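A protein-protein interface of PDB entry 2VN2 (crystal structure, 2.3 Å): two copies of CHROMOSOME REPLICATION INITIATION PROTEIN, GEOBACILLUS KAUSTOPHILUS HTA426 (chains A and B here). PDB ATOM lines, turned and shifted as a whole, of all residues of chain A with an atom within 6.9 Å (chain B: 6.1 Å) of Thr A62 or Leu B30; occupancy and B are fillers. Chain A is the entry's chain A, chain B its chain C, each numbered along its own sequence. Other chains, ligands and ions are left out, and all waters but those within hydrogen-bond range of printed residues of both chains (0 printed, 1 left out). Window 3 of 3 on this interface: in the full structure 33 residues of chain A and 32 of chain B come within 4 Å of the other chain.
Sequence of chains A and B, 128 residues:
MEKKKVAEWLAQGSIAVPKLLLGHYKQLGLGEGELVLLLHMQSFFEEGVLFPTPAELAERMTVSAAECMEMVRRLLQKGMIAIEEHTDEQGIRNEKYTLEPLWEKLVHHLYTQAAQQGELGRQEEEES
Of the 16 printed residues of chain B, 4 touch a printed residue of chain A.
Among the printed residues, 7 pairs touch across the chains.
Among the printed residues, no Asp or Glu carboxylate lies within 4 Å of a Lys or Arg side-chain nitrogen of the other chain.
The guanidinium group of Arg A60 lies within hydrogen-bond range of a ring nitrogen (ND1) of His A40.
The backbone carbonyl oxygen (O) of Tyr B25 sits at hydrogen-bond distance from the backbone NH (N) of Leu B30 (3.0 Å).
OE2 of Glu B32 lies within hydrogen-bond range of OH of Tyr B25, at 2.7 Å.
Of the printed residues of chain B, His A40 touches Tyr B25 (3.0 Å).
Printed residues of chain B within 4 Å of Arg A60: Tyr B25 (3.2 Å).
Of chain B, only Leu B30 (3.7 Å) and Glu B32 (2.7 Å) come within 4 Å of Thr A62.
Val A63 touches none of the printed residues of chain B.
No residue of chain A comes within 4 Å of Gly B29.
Of chain A, only Thr A62 comes within 4 Å of Leu B30.
The nearest printed residue of chain B that does not touch Thr A62 is Lys B26 (4.1 Å).
The nearest residue of chain A that does not touch Leu B30 is Met A61 (6.8 Å).
The nearest printed residue of chain A that does not touch Tyr B25 is Thr A62 (4.5 Å).
A ring nitrogen (NE2) of His A40 lies within hydrogen-bond range of the side-chain hydroxyl (OH) of Tyr B25.
O of Arg A60 sits at hydrogen-bond distance from OH of Tyr B25 (3.2 Å).
The side-chain hydroxyl (OG1) of Thr A62 lies within hydrogen-bond range of the side-chain carboxylate (OE1) of Glu B32 (2.7 Å).
Met A61 touches Tyr B25.
Met A61 touches Lys B26 (O to CD, 3.5 Å).
Met A61 touches Glu B32 (CB to OE2, 3.2 Å).
CG2 of Thr A62 touches O of Leu B30, at 3.7 Å.
No position is printed for both chains.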
ATOM      1  N   HIS A  40      -9.331  -1.117  31.466  1.00  0.00           N
ATOM      2  CA  HIS A  40     -10.036   0.239  31.331  1.00  0.00           C
ATOM      3  C   HIS A  40      -9.765   1.144  32.575  1.00  0.00           C
ATOM      4  O   HIS A  40      -9.557   2.344  32.391  1.00  0.00           O
ATOM      5  CB  HIS A  40     -11.520   0.229  31.053  1.00  0.00           C
ATOM      6  CG  HIS A  40     -11.917  -0.400  29.756  1.00  0.00           C
ATOM      7  ND1 HIS A  40     -11.791   0.225  28.539  1.00  0.00           N
ATOM      8  CD2 HIS A  40     -12.447  -1.617  29.498  1.00  0.00           C
ATOM      9  CE1 HIS A  40     -12.222  -0.579  27.585  1.00  0.00           C
ATOM     10  NE2 HIS A  40     -12.621  -1.703  28.145  1.00  0.00           N
ATOM     11  N   ALA A  58     -18.362   1.147  31.761  1.00  0.00           N
ATOM     12  CA  ALA A  58     -19.152   0.256  30.848  1.00  0.00           C
ATOM     13  C   ALA A  58     -19.212   0.735  29.414  1.00  0.00           C
ATOM     14  O   ALA A  58     -19.529  -0.063  28.504  1.00  0.00           O
ATOM     15  CB  ALA A  58     -20.590   0.036  31.355  1.00  0.00           C
ATOM     16  N   GLU A  59     -18.896   2.022  29.215  1.00  0.00           N
ATOM     17  CA  GLU A  59     -19.141   2.744  27.959  1.00  0.00           C
ATOM     18  C   GLU A  59     -18.261   2.148  26.905  1.00  0.00           C
ATOM     19  O   GLU A  59     -18.696   2.067  25.777  1.00  0.00           O
ATOM     20  CB  GLU A  59     -18.952   4.300  28.095  1.00  0.00           C
ATOM     21  CG  GLU A  59     -17.629   4.964  27.535  1.00  0.00           C
ATOM     22  CD  GLU A  59     -17.254   6.428  28.178  1.00  0.00           C
ATOM     23  OE1 GLU A  59     -18.225   7.197  28.494  1.00  0.00           O
ATOM     24  OE2 GLU A  59     -16.025   6.791  28.367  1.00  0.00           O
ATOM     25  N   ARG A  60     -17.042   1.707  27.265  1.00  0.00           N
ATOM     26  CA  ARG A  60     -16.104   1.050  26.300  1.00  0.00           C
ATOM     27  C   ARG A  60     -16.117  -0.483  26.384  1.00  0.00           C
ATOM     28  O   ARG A  60     -15.307  -1.127  25.783  1.00  0.00           O
ATOM     29  CB  ARG A  60     -14.665   1.653  26.392  1.00  0.00           C
ATOM     30  CG  ARG A  60     -14.559   3.265  26.356  1.00  0.00           C
ATOM     31  CD  ARG A  60     -13.048   3.833  26.356  1.00  0.00           C
ATOM     32  NE  ARG A  60     -12.417   4.265  27.647  1.00  0.00           N
ATOM     33  CZ  ARG A  60     -11.317   3.769  28.323  1.00  0.00           C
ATOM     34  NH1 ARG A  60     -10.552   2.672  27.969  1.00  0.00           N
ATOM     35  NH2 ARG A  60     -10.970   4.434  29.454  1.00  0.00           N
ATOM     36  N   MET A  61     -17.061  -1.090  27.119  1.00  0.00           N
ATOM     37  CA  MET A  61     -17.079  -2.567  27.286  1.00  0.00           C
ATOM     38  C   MET A  61     -18.377  -3.117  26.666  1.00  0.00           C
ATOM     39  O   MET A  61     -19.316  -2.349  26.428  1.00  0.00           O
ATOM     40  CB  MET A  61     -17.020  -3.025  28.773  1.00  0.00           C
ATOM     41  CG  MET A  61     -16.111  -2.400  29.621  1.00  0.00           C
ATOM     42  SD  MET A  61     -15.740  -3.111  31.301  1.00  0.00           S
ATOM     43  CE  MET A  61     -15.660  -1.505  31.508  1.00  0.00           C
ATOM     44  N   THR A  62     -18.463  -4.426  26.481  1.00  0.00           N
ATOM     45  CA  THR A  62     -19.702  -5.014  25.985  1.00  0.00           C
ATOM     46  C   THR A  62     -20.770  -5.239  27.087  1.00  0.00           C
ATOM     47  O   THR A  62     -21.889  -5.705  26.777  1.00  0.00           O
ATOM     48  CB  THR A  62     -19.465  -6.371  25.362  1.00  0.00           C
ATOM     49  OG1 THR A  62     -18.960  -7.226  26.389  1.00  0.00           O
ATOM     50  CG2 THR A  62     -18.502  -6.287  24.116  1.00  0.00           C
ATOM     51  N   VAL A  63     -20.440  -4.963  28.351  1.00  0.00           N
ATOM     52  CA  VAL A  63     -21.354  -5.151  29.445  1.00  0.00           C
ATOM     53  C   VAL A  63     -22.156  -3.844  29.868  1.00  0.00           C
ATOM     54  O   VAL A  63     -21.665  -2.733  29.643  1.00  0.00           O
ATOM     55  CB  VAL A  63     -20.626  -5.778  30.669  1.00  0.00           C
ATOM     56  CG1 VAL A  63     -20.021  -7.102  30.243  1.00  0.00           C
ATOM     57  CG2 VAL A  63     -19.603  -4.913  31.185  1.00  0.00           C
ATOM     58  N   SER A  64     -23.330  -3.988  30.490  1.00  0.00           N
ATOM     59  CA  SER A  64     -24.048  -2.864  30.975  1.00  0.00           C
ATOM     60  C   SER A  64     -23.360  -2.236  32.180  1.00  0.00           C
ATOM     61  O   SER A  64     -22.439  -2.791  32.823  1.00  0.00           O
ATOM     62  CB  SER A  64     -25.496  -3.299  31.363  1.00  0.00           C
ATOM     63  OG  SER A  64     -25.457  -4.199  32.467  1.00  0.00           O
ATOM     64  N   GLU A  67     -23.821  -4.434  35.193  1.00  0.00           N
ATOM     65  CA  GLU A  67     -22.896  -5.617  35.238  1.00  0.00           C
ATOM     66  C   GLU A  67     -21.556  -5.160  35.660  1.00  0.00           C
ATOM     67  O   GLU A  67     -20.952  -5.739  36.530  1.00  0.00           O
ATOM     68  CB  GLU A  67     -22.777  -6.289  33.864  1.00  0.00           C
ATOM     69  CG  GLU A  67     -24.070  -6.926  33.393  1.00  0.00           C
ATOM     70  CD  GLU A  67     -24.076  -7.408  31.913  1.00  0.00           C
ATOM     71  OE1 GLU A  67     -23.758  -8.625  31.782  1.00  0.00           O
ATOM     72  OE2 GLU A  67     -24.394  -6.641  30.906  1.00  0.00           O
ATOM     73  N   LEU B  21      -7.100   0.787  20.555  1.00  0.00           N
ATOM     74  CA  LEU B  21      -7.711  -0.482  20.604  1.00  0.00           C
ATOM     75  C   LEU B  21      -8.598  -0.638  21.857  1.00  0.00           C
ATOM     76  O   LEU B  21      -9.812  -1.012  21.741  1.00  0.00           O
ATOM     77  CB  LEU B  21      -6.723  -1.644  20.499  1.00  0.00           C
ATOM     78  CG  LEU B  21      -7.220  -3.095  20.402  1.00  0.00           C
ATOM     79  CD1 LEU B  21      -8.265  -3.237  19.216  1.00  0.00           C
ATOM     80  CD2 LEU B  21      -5.986  -4.004  20.202  1.00  0.00           C
ATOM     81  N   TYR B  25     -12.460  -1.585  20.585  1.00  0.00           N
ATOM     82  CA  TYR B  25     -12.640  -2.985  20.274  1.00  0.00           C
ATOM     83  C   TYR B  25     -14.127  -3.371  20.231  1.00  0.00           C
ATOM     84  O   TYR B  25     -14.504  -4.186  19.455  1.00  0.00           O
ATOM     85  CB  TYR B  25     -11.841  -3.870  21.217  1.00  0.00           C
ATOM     86  CG  TYR B  25     -12.398  -3.901  22.654  1.00  0.00           C
ATOM     87  CD1 TYR B  25     -13.385  -4.797  23.025  1.00  0.00           C
ATOM     88  CD2 TYR B  25     -11.926  -2.997  23.643  1.00  0.00           C
ATOM     89  CE1 TYR B  25     -13.924  -4.816  24.294  1.00  0.00           C
ATOM     90  CE2 TYR B  25     -12.471  -2.994  24.946  1.00  0.00           C
ATOM     91  CZ  TYR B  25     -13.443  -3.924  25.268  1.00  0.00           C
ATOM     92  OH  TYR B  25     -13.943  -3.919  26.540  1.00  0.00           O
ATOM     93  N   LYS B  26     -14.984  -2.752  21.025  1.00  0.00           N
ATOM     94  CA  LYS B  26     -16.373  -3.233  21.177  1.00  0.00           C
ATOM     95  C   LYS B  26     -17.076  -2.866  19.870  1.00  0.00           C
ATOM     96  O   LYS B  26     -17.829  -3.691  19.349  1.00  0.00           O
ATOM     97  CB  LYS B  26     -17.070  -2.656  22.431  1.00  0.00           C
ATOM     98  CG  LYS B  26     -18.627  -2.593  22.371  1.00  0.00           C
ATOM     99  CD  LYS B  26     -19.228  -1.280  23.055  1.00  0.00           C
ATOM    100  CE  LYS B  26     -20.800  -1.241  22.760  1.00  0.00           C
ATOM    101  NZ  LYS B  26     -21.403  -2.669  22.655  1.00  0.00           N
ATOM    102  N   GLN B  27     -16.766  -1.682  19.321  1.00  0.00           N
ATOM    103  CA  GLN B  27     -17.242  -1.298  18.015  1.00  0.00           C
ATOM    104  C   GLN B  27     -16.764  -2.131  16.823  1.00  0.00           C
ATOM    105  O   GLN B  27     -17.428  -2.120  15.832  1.00  0.00           O
ATOM    106  CB  GLN B  27     -16.979   0.156  17.743  1.00  0.00           C
ATOM    107  CG  GLN B  27     -17.778   1.167  18.611  1.00  0.00           C
ATOM    108  CD  GLN B  27     -16.855   2.306  19.048  1.00  0.00           C
ATOM    109  OE1 GLN B  27     -17.262   3.490  19.146  1.00  0.00           O
ATOM    110  NE2 GLN B  27     -15.584   1.979  19.236  1.00  0.00           N
ATOM    111  N   LEU B  28     -15.654  -2.869  16.937  1.00  0.00           N
ATOM    112  CA  LEU B  28     -15.084  -3.641  15.894  1.00  0.00           C
ATOM    113  C   LEU B  28     -15.758  -4.978  16.049  1.00  0.00           C
ATOM    114  O   LEU B  28     -15.536  -5.937  15.305  1.00  0.00           O
ATOM    115  CB  LEU B  28     -13.585  -3.764  16.143  1.00  0.00           C
ATOM    116  CG  LEU B  28     -12.402  -3.018  15.422  1.00  0.00           C
ATOM    117  CD1 LEU B  28     -12.769  -1.751  14.547  1.00  0.00           C
ATOM    118  CD2 LEU B  28     -11.054  -2.784  16.271  1.00  0.00           C
ATOM    119  N   GLY B  29     -16.635  -5.100  17.041  1.00  0.00           N
ATOM    120  CA  GLY B  29     -17.389  -6.347  17.088  1.00  0.00           C
ATOM    121  C   GLY B  29     -16.619  -7.336  17.934  1.00  0.00           C
ATOM    122  O   GLY B  29     -16.913  -8.495  17.851  1.00  0.00           O
ATOM    123  N   LEU B  30     -15.619  -6.889  18.728  1.00  0.00           N
ATOM    124  CA  LEU B  30     -14.849  -7.802  19.568  1.00  0.00           C
ATOM    125  C   LEU B  30     -15.372  -7.809  21.001  1.00  0.00           C
ATOM    126  O   LEU B  30     -15.891  -6.790  21.517  1.00  0.00           O
ATOM    127  CB  LEU B  30     -13.336  -7.495  19.570  1.00  0.00           C
ATOM    128  CG  LEU B  30     -12.643  -7.552  18.219  1.00  0.00           C
ATOM    129  CD1 LEU B  30     -11.456  -6.590  18.293  1.00  0.00           C
ATOM    130  CD2 LEU B  30     -12.122  -8.897  18.108  1.00  0.00           C
ATOM    131  N   GLY B  31     -15.281  -8.938  21.643  1.00  0.00           N
ATOM    132  CA  GLY B  31     -15.600  -8.967  23.048  1.00  0.00           C
ATOM    133  C   GLY B  31     -14.314  -8.930  23.902  1.00  0.00           C
ATOM    134  O   GLY B  31     -13.200  -9.127  23.355  1.00  0.00           O
ATOM    135  N   GLU B  32     -14.456  -8.701  25.235  1.00  0.00           N
ATOM    136  CA  GLU B  32     -13.303  -8.764  26.203  1.00  0.00           C
ATOM    137  C   GLU B  32     -12.570 -10.087  26.076  1.00  0.00           C
ATOM    138  O   GLU B  32     -11.373 -10.164  26.116  1.00  0.00           O
ATOM    139  CB  GLU B  32     -13.830  -8.566  27.647  1.00  0.00           C
ATOM    140  CG  GLU B  32     -14.318  -7.140  28.041  1.00  0.00           C
ATOM    141  CD  GLU B  32     -15.664  -6.783  27.447  1.00  0.00           C
ATOM    142  OE1 GLU B  32     -16.463  -7.728  27.222  1.00  0.00           O
ATOM    143  OE2 GLU B  32     -15.959  -5.552  27.203  1.00  0.00           O
ATOM    144  N   GLU B  34     -12.107 -11.973  23.504  1.00  0.00           N
ATOM    145  CA  GLU B  34     -11.376 -12.035  22.243  1.00  0.00           C
ATOM    146  C   GLU B  34     -10.203 -11.047  22.392  1.00  0.00           C
ATOM    147  O   GLU B  34      -9.061 -11.451  22.176  1.00  0.00           O
ATOM    148  CB  GLU B  34     -12.256 -11.681  21.023  1.00  0.00           C
ATOM    149  CG  GLU B  34     -13.276 -12.802  20.524  1.00  0.00           C
ATOM    150  CD  GLU B  34     -14.345 -12.168  19.608  1.00  0.00           C
ATOM    151  OE1 GLU B  34     -14.904 -11.077  19.920  1.00  0.00           O
ATOM    152  OE2 GLU B  34     -14.621 -12.702  18.527  1.00  0.00           O
ATOM    153  N   LEU B  35     -10.470  -9.829  22.845  1.00  0.00           N
ATOM    154  CA  LEU B  35      -9.408  -8.903  23.240  1.00  0.00           C
ATOM    155  C   LEU B  35      -8.240  -9.604  24.028  1.00  0.00           C
ATOM    156  O   LEU B  35      -7.058  -9.608  23.557  1.00  0.00           O
ATOM    157  CB  LEU B  35      -9.959  -7.639  23.965  1.00  0.00           C
ATOM    158  CG  LEU B  35      -8.901  -6.586  24.307  1.00  0.00           C
ATOM    159  CD1 LEU B  35      -8.280  -6.045  22.927  1.00  0.00           C
ATOM    160  CD2 LEU B  35      -9.494  -5.383  25.057  1.00  0.00           C
ATOM    161  N   LEU B  38      -6.330 -12.011  21.944  1.00  0.00           N
ATOM    162  CA  LEU B  38      -5.316 -11.179  21.104  1.00  0.00           C
ATOM    163  C   LEU B  38      -4.077 -10.768  21.954  1.00  0.00           C
ATOM    164  O   LEU B  38      -2.953 -10.748  21.461  1.00  0.00           O
ATOM    165  CB  LEU B  38      -5.985  -9.898  20.522  1.00  0.00           C
ATOM    166  CG  LEU B  38      -7.186 -10.082  19.516  1.00  0.00           C
ATOM    167  CD1 LEU B  38      -7.922  -8.832  19.162  1.00  0.00           C
ATOM    168  CD2 LEU B  38      -6.768 -10.771  18.201  1.00  0.00           C
ATOM    169  N   LEU B  75     -12.381 -15.093  14.920  1.00  0.00           N
ATOM    170  CA  LEU B  75     -11.530 -13.938  14.606  1.00  0.00           C
ATOM    171  C   LEU B  75     -11.110 -13.982  13.128  1.00  0.00           C
ATOM    172  O   LEU B  75     -11.104 -12.956  12.452  1.00  0.00           O
ATOM    173  CB  LEU B  75     -10.311 -13.753  15.543  1.00  0.00           C
ATOM    174  CG  LEU B  75     -10.633 -13.326  16.997  1.00  0.00           C
ATOM    175  CD1 LEU B  75      -9.316 -13.420  17.853  1.00  0.00           C
ATOM    176  CD2 LEU B  75     -11.294 -11.946  17.087  1.00  0.00           C
ATOM    177  N   LYS B  78     -14.137 -12.821  11.059  1.00  0.00           N
ATOM    178  CA  LYS B  78     -14.315 -11.385  11.191  1.00  0.00           C
ATOM    179  C   LYS B  78     -13.252 -10.575  10.451  1.00  0.00           C
ATOM    180  O   LYS B  78     -13.387  -9.332  10.325  1.00  0.00           O
ATOM    181  CB  LYS B  78     -14.294 -11.017  12.676  1.00  0.00           C
ATOM    182  CG  LYS B  78     -15.599 -11.452  13.425  1.00  0.00           C
ATOM    183  CD  LYS B  78     -15.435 -11.463  14.941  1.00  0.00           C
ATOM    184  CE  LYS B  78     -16.804 -11.464  15.593  1.00  0.00           C
ATOM    185  NZ  LYS B  78     -16.574 -11.431  17.029  1.00  0.00           N
ATOM    186  N   MET B  80     -10.106 -10.207  11.716  1.00  0.00           N
ATOM    187  CA  MET B  80      -9.363  -9.499  12.758  1.00  0.00           C
ATOM    188  C   MET B  80      -7.956 -10.009  12.826  1.00  0.00           C
ATOM    189  O   MET B  80      -7.064  -9.290  13.208  1.00  0.00           O
ATOM    190  CB  MET B  80     -10.084  -9.582  14.121  1.00  0.00           C
ATOM    191  CG  MET B  80     -11.415  -8.827  14.075  1.00  0.00           C
ATOM    192  SD  MET B  80     -11.321  -7.045  14.086  1.00  0.00           S
ATOM    193  CE  MET B  80     -12.882  -7.059  13.190  1.00  0.00           C
ATOM    194  N   LEU B 102      -6.363  -6.570  12.091  1.00  0.00           N
ATOM    195  CA  LEU B 102      -6.997  -5.807  13.200  1.00  0.00           C
ATOM    196  C   LEU B 102      -6.721  -4.329  13.008  1.00  0.00           C
ATOM    197  O   LEU B 102      -7.600  -3.496  13.135  1.00  0.00           O
ATOM    198  CB  LEU B 102      -6.383  -6.234  14.555  1.00  0.00           C
ATOM    199  CG  LEU B 102      -6.890  -5.734  15.897  1.00  0.00           C
ATOM    200  CD1 LEU B 102      -8.307  -6.264  16.127  1.00  0.00           C
ATOM    201  CD2 LEU B 102      -5.924  -6.246  17.047  1.00  0.00           C
